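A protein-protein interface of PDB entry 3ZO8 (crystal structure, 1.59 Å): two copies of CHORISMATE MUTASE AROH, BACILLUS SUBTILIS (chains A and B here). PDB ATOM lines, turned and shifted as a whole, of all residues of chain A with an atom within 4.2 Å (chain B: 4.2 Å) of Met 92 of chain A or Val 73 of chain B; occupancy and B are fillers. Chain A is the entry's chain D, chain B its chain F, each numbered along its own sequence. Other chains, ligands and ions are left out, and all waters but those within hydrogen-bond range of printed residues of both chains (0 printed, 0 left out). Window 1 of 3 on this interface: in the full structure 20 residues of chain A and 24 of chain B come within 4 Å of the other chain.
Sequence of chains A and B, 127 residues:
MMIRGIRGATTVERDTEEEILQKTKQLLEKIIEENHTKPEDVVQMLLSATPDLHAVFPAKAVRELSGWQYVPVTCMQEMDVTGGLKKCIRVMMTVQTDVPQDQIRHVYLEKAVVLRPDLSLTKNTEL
Ile 6 of chain A touches none of the printed residues of chain B. Of the printed residues of chain B, Arg 7 of chain A touches Pro 72, Val 73 and Thr 74. Printed residues of chain A within 4 Å of Gln 44 of chain B: Gly 5 (3.8 Å), Met 92 (3.8 Å) and Thr 94 (2.6 Å). Of the printed residues of chain A, Met 45 of chain B touches Met 92 (3.9 Å). Of the printed residues of chain A, Pro 72 of chain B touches Gly 5, Arg 7 and Met 92. Of chain A, only Arg 7 and Met 92 come within 4 Å of Val 73 of chain B. Of the printed residues of chain A, Thr 74 of chain B touches Arg 7 (3.9 Å) and Met 92 (3.8 Å). The nearest printed residue of chain A that does not touch Val 73 of chain B is Val 91 of chain A (6.8 Å). The nearest printed residue of chain B that does not touch Arg 7 of chain A is Arg 63 of chain B (5.6 Å).
The backbone carbonyl oxygen (O) of Met 45 of chain B is in hydrogen-bond range of the backbone NH (N) of Thr 74 of chain B, 3.2 Å away. The guanidinium group (NE) of Arg 7 of chain A sits at hydrogen-bond distance from the backbone carbonyl oxygen (O) of Val 91 of chain A (2.9 Å). N of Met 45 of chain B is in hydrogen-bond range of O of Pro 72 of chain B, at 2.9 Å. The backbone carbonyl oxygen of Thr 74 of chain B lies within hydrogen-bond range of the backbone NH of Leu 47 of chain B, at 3.1 Å. The backbone carbonyl oxygen of Leu 46 of chain A sits at hydrogen-bond distance from the backbone NH of Met 92 of chain A (2.9 Å).
Position printed for both chains: 45. Of the 11 pairs that touch across the chains among the printed residues, none has its exchanged pair printed and touching as well.
Of the 9 printed residues of chain B, 5 touch a printed residue of chain A. Hydrophobic or aromatic side chains of chain B that line the printed part of chain A: Pro 72. Of the 9 printed residues of chain A, 4 touch a printed residue of chain B. Printed residues of chain A that touch a printed residue of chain B: Gly 5, Arg 7, Met 92 and Thr 94. Among the printed residues, no Asp or Glu carboxylate lies within 4 Å of a Lys or Arg side-chain nitrogen of the other chain.
CA of Gly 5 of chain A touches OE1 of Gln 44 of chain B, 3.8 Å away. Gly 5 of chain A touches Pro 72 of chain B. Pro 72 of chain B touches Arg 7 of chain A. Arg 7 of chain A touches Thr 74 of chain B. CG of Met 92 of chain A touches OE1 of Gln 44 of chain B (3.8 Å). Met 45 of chain B touches Met 92 of chain A (O to CE, 3.9 Å). Pro 72 of chain B touches Met 92 of chain A. CE of Met 92 of chain A touches CA of Val 73 of chain B, 3.97 Å away. Thr 74 of chain B touches Met 92 of chain A (CG2 to CE, 3.8 Å).
NH1 of Arg 7 of chain A lies within hydrogen-bond range of O of Val 73 of chain B (3.0 Å). The side-chain amide oxygen (OE1) of Gln 44 of chain B sits at hydrogen-bond distance from the side-chain hydroxyl (OG1) of Thr 94 of chain A (2.6 Å).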
ATOM      1  N   GLY A   5     -13.369 -26.502  20.979  1.00  0.00           N
ATOM      2  CA  GLY A   5     -14.253 -27.651  21.099  1.00  0.00           C
ATOM      3  C   GLY A   5     -13.858 -28.774  20.156  1.00  0.00           C
ATOM      4  O   GLY A   5     -13.516 -28.536  18.997  1.00  0.00           O
ATOM      5  N   ILE A   6     -13.907 -29.999  20.666  1.00  0.00           N
ATOM      6  CA  ILE A   6     -13.684 -31.193  19.862  1.00  0.00           C
ATOM      7  C   ILE A   6     -14.953 -32.023  19.829  1.00  0.00           C
ATOM      8  O   ILE A   6     -15.533 -32.339  20.871  1.00  0.00           O
ATOM      9  CB  ILE A   6     -12.588 -32.086  20.442  1.00  0.00           C
ATOM     10  CG1 ILE A   6     -11.343 -31.245  20.744  1.00  0.00           C
ATOM     11  CG2 ILE A   6     -12.324 -33.240  19.479  1.00  0.00           C
ATOM     12  CD1 ILE A   6     -10.128 -32.021  21.208  1.00  0.00           C
ATOM     13  N   ARG A   7     -15.379 -32.368  18.628  1.00  0.00           N
ATOM     14  CA  ARG A   7     -16.646 -33.051  18.440  1.00  0.00           C
ATOM     15  C   ARG A   7     -16.410 -34.518  18.153  1.00  0.00           C
ATOM     16  O   ARG A   7     -15.476 -34.877  17.433  1.00  0.00           O
ATOM     17  CB  ARG A   7     -17.426 -32.434  17.275  1.00  0.00           C
ATOM     18  CG  ARG A   7     -18.145 -31.134  17.585  1.00  0.00           C
ATOM     19  CD  ARG A   7     -19.354 -31.358  18.486  1.00  0.00           C
ATOM     20  NE  ARG A   7     -19.947 -32.687  18.340  1.00  0.00           N
ATOM     21  CZ  ARG A   7     -20.707 -33.079  17.320  1.00  0.00           C
ATOM     22  NH1 ARG A   7     -20.980 -32.250  16.322  1.00  0.00           N
ATOM     23  NH2 ARG A   7     -21.190 -34.313  17.294  1.00  0.00           N
ATOM     24  N   MET A  45     -16.923 -31.181  29.513  1.00  0.00           N
ATOM     25  CA  MET A  45     -17.393 -32.030  28.433  1.00  0.00           C
ATOM     26  C   MET A  45     -18.913 -32.099  28.488  1.00  0.00           C
ATOM     27  O   MET A  45     -19.501 -32.194  29.576  1.00  0.00           O
ATOM     28  CB  MET A  45     -16.776 -33.423  28.579  1.00  0.00           C
ATOM     29  CG  MET A  45     -17.175 -34.461  27.543  1.00  0.00           C
ATOM     30  SD  MET A  45     -16.346 -36.026  27.922  1.00  0.00           S
ATOM     31  CE  MET A  45     -14.690 -35.427  28.223  1.00  0.00           C
ATOM     32  N   LEU A  46     -19.542 -32.016  27.318  1.00  0.00           N
ATOM     33  CA  LEU A  46     -20.979 -32.282  27.193  1.00  0.00           C
ATOM     34  C   LEU A  46     -21.217 -33.544  26.377  1.00  0.00           C
ATOM     35  O   LEU A  46     -20.636 -33.717  25.315  1.00  0.00           O
ATOM     36  CB  LEU A  46     -21.684 -31.109  26.521  1.00  0.00           C
ATOM     37  CG  LEU A  46     -21.545 -29.772  27.247  1.00  0.00           C
ATOM     38  CD1 LEU A  46     -22.281 -28.684  26.483  1.00  0.00           C
ATOM     39  CD2 LEU A  46     -22.061 -29.886  28.676  1.00  0.00           C
ATOM     40  N   VAL A  91     -20.352 -36.143  21.479  1.00  0.00           N
ATOM     41  CA  VAL A  91     -19.606 -35.418  22.492  1.00  0.00           C
ATOM     42  C   VAL A  91     -19.208 -34.023  22.012  1.00  0.00           C
ATOM     43  O   VAL A  91     -19.049 -33.800  20.813  1.00  0.00           O
ATOM     44  CB  VAL A  91     -18.378 -36.215  22.988  1.00  0.00           C
ATOM     45  CG1 VAL A  91     -17.598 -36.802  21.824  1.00  0.00           C
ATOM     46  CG2 VAL A  91     -17.491 -35.339  23.861  1.00  0.00           C
ATOM     47  N   MET A  92     -19.120 -33.087  22.959  1.00  0.00           N
ATOM     48  CA  MET A  92     -18.385 -31.834  22.786  1.00  0.00           C
ATOM     49  C   MET A  92     -17.391 -31.705  23.933  1.00  0.00           C
ATOM     50  O   MET A  92     -17.767 -31.460  25.080  1.00  0.00           O
ATOM     51  CB  MET A  92     -19.294 -30.598  22.743  1.00  0.00           C
ATOM     52  CG  MET A  92     -18.531 -29.285  22.612  1.00  0.00           C
ATOM     53  SD  MET A  92     -18.110 -28.875  20.907  1.00  0.00           S
ATOM     54  CE  MET A  92     -19.740 -28.439  20.288  1.00  0.00           C
ATOM     55  N   MET A  93     -16.121 -31.920  23.618  1.00  0.00           N
ATOM     56  CA  MET A  93     -15.043 -31.783  24.587  1.00  0.00           C
ATOM     57  C   MET A  93     -14.366 -30.429  24.391  1.00  0.00           C
ATOM     58  O   MET A  93     -13.847 -30.137  23.310  1.00  0.00           O
ATOM     59  CB  MET A  93     -14.019 -32.904  24.385  1.00  0.00           C
ATOM     60  CG  MET A  93     -12.918 -33.002  25.434  1.00  0.00           C
ATOM     61  SD  MET A  93     -11.769 -34.307  24.942  1.00  0.00           S
ATOM     62  CE  MET A  93     -12.994 -35.488  24.395  1.00  0.00           C
ATOM     63  N   THR A  94     -14.380 -29.600  25.429  1.00  0.00           N
ATOM     64  CA  THR A  94     -13.759 -28.282  25.354  1.00  0.00           C
ATOM     65  C   THR A  94     -12.386 -28.355  26.008  1.00  0.00           C
ATOM     66  O   THR A  94     -12.270 -28.716  27.184  1.00  0.00           O
ATOM     67  CB  THR A  94     -14.623 -27.216  26.057  1.00  0.00           C
ATOM     68  OG1 THR A  94     -15.977 -27.314  25.592  1.00  0.00           O
ATOM     69  CG2 THR A  94     -14.072 -25.806  25.793  1.00  0.00           C
ATOM     70  N   GLN B  44     -16.720 -22.802  20.364  1.00  0.00           N
ATOM     71  CA  GLN B  44     -17.731 -23.789  19.998  1.00  0.00           C
ATOM     72  C   GLN B  44     -19.097 -23.132  20.059  1.00  0.00           C
ATOM     73  O   GLN B  44     -19.229 -22.014  20.570  1.00  0.00           O
ATOM     74  CB  GLN B  44     -17.717 -24.967  20.968  1.00  0.00           C
ATOM     75  CG  GLN B  44     -18.338 -24.648  22.320  1.00  0.00           C
ATOM     76  CD  GLN B  44     -17.889 -25.600  23.411  1.00  0.00           C
ATOM     77  OE1 GLN B  44     -16.747 -26.052  23.422  1.00  0.00           O
ATOM     78  NE2 GLN B  44     -18.791 -25.918  24.334  1.00  0.00           N
ATOM     79  N   MET B  45     -20.105 -23.846  19.562  1.00  0.00           N
ATOM     80  CA  MET B  45     -21.470 -23.346  19.507  1.00  0.00           C
ATOM     81  C   MET B  45     -22.442 -24.429  19.947  1.00  0.00           C
ATOM     82  O   MET B  45     -22.301 -25.585  19.577  1.00  0.00           O
ATOM     83  CB  MET B  45     -21.836 -22.928  18.083  1.00  0.00           C
ATOM     84  CG  MET B  45     -21.358 -21.554  17.654  1.00  0.00           C
ATOM     85  SD  MET B  45     -21.975 -21.200  15.996  1.00  0.00           S
ATOM     86  CE  MET B  45     -23.677 -21.731  16.146  1.00  0.00           C
ATOM     87  N   LEU B  47     -26.636 -25.113  19.923  1.00  0.00           N
ATOM     88  CA  LEU B  47     -27.951 -24.655  19.512  1.00  0.00           C
ATOM     89  C   LEU B  47     -28.974 -25.617  20.077  1.00  0.00           C
ATOM     90  O   LEU B  47     -28.744 -26.830  20.105  1.00  0.00           O
ATOM     91  CB  LEU B  47     -28.067 -24.570  17.990  1.00  0.00           C
ATOM     92  CG  LEU B  47     -27.013 -23.706  17.298  1.00  0.00           C
ATOM     93  CD1 LEU B  47     -25.840 -24.593  16.917  1.00  0.00           C
ATOM     94  CD2 LEU B  47     -27.588 -22.978  16.083  1.00  0.00           C
ATOM     95  N   ALA B  59     -27.936 -26.783  13.277  1.00  0.00           N
ATOM     96  CA  ALA B  59     -26.483 -26.745  13.047  1.00  0.00           C
ATOM     97  C   ALA B  59     -26.103 -26.690  11.576  1.00  0.00           C
ATOM     98  O   ALA B  59     -24.996 -26.277  11.224  1.00  0.00           O
ATOM     99  CB  ALA B  59     -25.811 -27.947  13.700  1.00  0.00           C
ATOM    100  N   ARG B  63     -23.174 -24.265   8.384  1.00  0.00           N
ATOM    101  CA  ARG B  63     -22.416 -24.737   7.230  1.00  0.00           C
ATOM    102  C   ARG B  63     -22.660 -23.872   5.991  1.00  0.00           C
ATOM    103  O   ARG B  63     -22.035 -24.074   4.950  1.00  0.00           O
ATOM    104  CB  ARG B  63     -22.772 -26.195   6.934  1.00  0.00           C
ATOM    105  CG  ARG B  63     -22.927 -27.054   8.181  1.00  0.00           C
ATOM    106  CD  ARG B  63     -21.584 -27.522   8.719  1.00  0.00           C
ATOM    107  NE  ARG B  63     -21.669 -27.950  10.114  1.00  0.00           N
ATOM    108  CZ  ARG B  63     -22.406 -28.970  10.542  1.00  0.00           C
ATOM    109  NH1 ARG B  63     -23.140 -29.667   9.684  1.00  0.00           N
ATOM    110  NH2 ARG B  63     -22.418 -29.288  11.830  1.00  0.00           N
ATOM    111  N   VAL B  71     -15.881 -24.626  12.653  1.00  0.00           N
ATOM    112  CA  VAL B  71     -16.420 -24.237  13.944  1.00  0.00           C
ATOM    113  C   VAL B  71     -17.187 -25.424  14.533  1.00  0.00           C
ATOM    114  O   VAL B  71     -18.094 -25.955  13.890  1.00  0.00           O
ATOM    115  CB  VAL B  71     -17.316 -22.985  13.828  1.00  0.00           C
ATOM    116  CG1 VAL B  71     -17.976 -22.670  15.162  1.00  0.00           C
ATOM    117  CG2 VAL B  71     -16.504 -21.789  13.342  1.00  0.00           C
ATOM    118  N   PRO B  72     -16.802 -25.876  15.742  1.00  0.00           N
ATOM    119  CA  PRO B  72     -17.489 -27.051  16.267  1.00  0.00           C
ATOM    120  C   PRO B  72     -18.860 -26.711  16.875  1.00  0.00           C
ATOM    121  O   PRO B  72     -18.972 -25.813  17.710  1.00  0.00           O
ATOM    122  CB  PRO B  72     -16.511 -27.592  17.319  1.00  0.00           C
ATOM    123  CG  PRO B  72     -15.769 -26.386  17.790  1.00  0.00           C
ATOM    124  CD  PRO B  72     -15.714 -25.419  16.629  1.00  0.00           C
ATOM    125  N   VAL B  73     -19.894 -27.419  16.435  1.00  0.00           N
ATOM    126  CA  VAL B  73     -21.260 -27.124  16.864  1.00  0.00           C
ATOM    127  C   VAL B  73     -22.088 -28.396  17.085  1.00  0.00           C
ATOM    128  O   VAL B  73     -21.886 -29.420  16.423  1.00  0.00           O
ATOM    129  CB  VAL B  73     -21.949 -26.113  15.904  1.00  0.00           C
ATOM    130  CG1 VAL B  73     -21.766 -26.498  14.440  1.00  0.00           C
ATOM    131  CG2 VAL B  73     -23.414 -25.929  16.254  1.00  0.00           C
ATOM    132  N   THR B  74     -22.997 -28.343  18.051  1.00  0.00           N
ATOM    133  CA  THR B  74     -23.863 -29.483  18.302  1.00  0.00           C
ATOM    134  C   THR B  74     -25.166 -29.010  18.912  1.00  0.00           C
ATOM    135  O   THR B  74     -25.266 -27.898  19.437  1.00  0.00           O
ATOM    136  CB  THR B  74     -23.201 -30.558  19.181  1.00  0.00           C
ATOM    137  OG1 THR B  74     -23.937 -31.788  19.079  1.00  0.00           O
ATOM    138  CG2 THR B  74     -23.133 -30.107  20.643  1.00  0.00           C
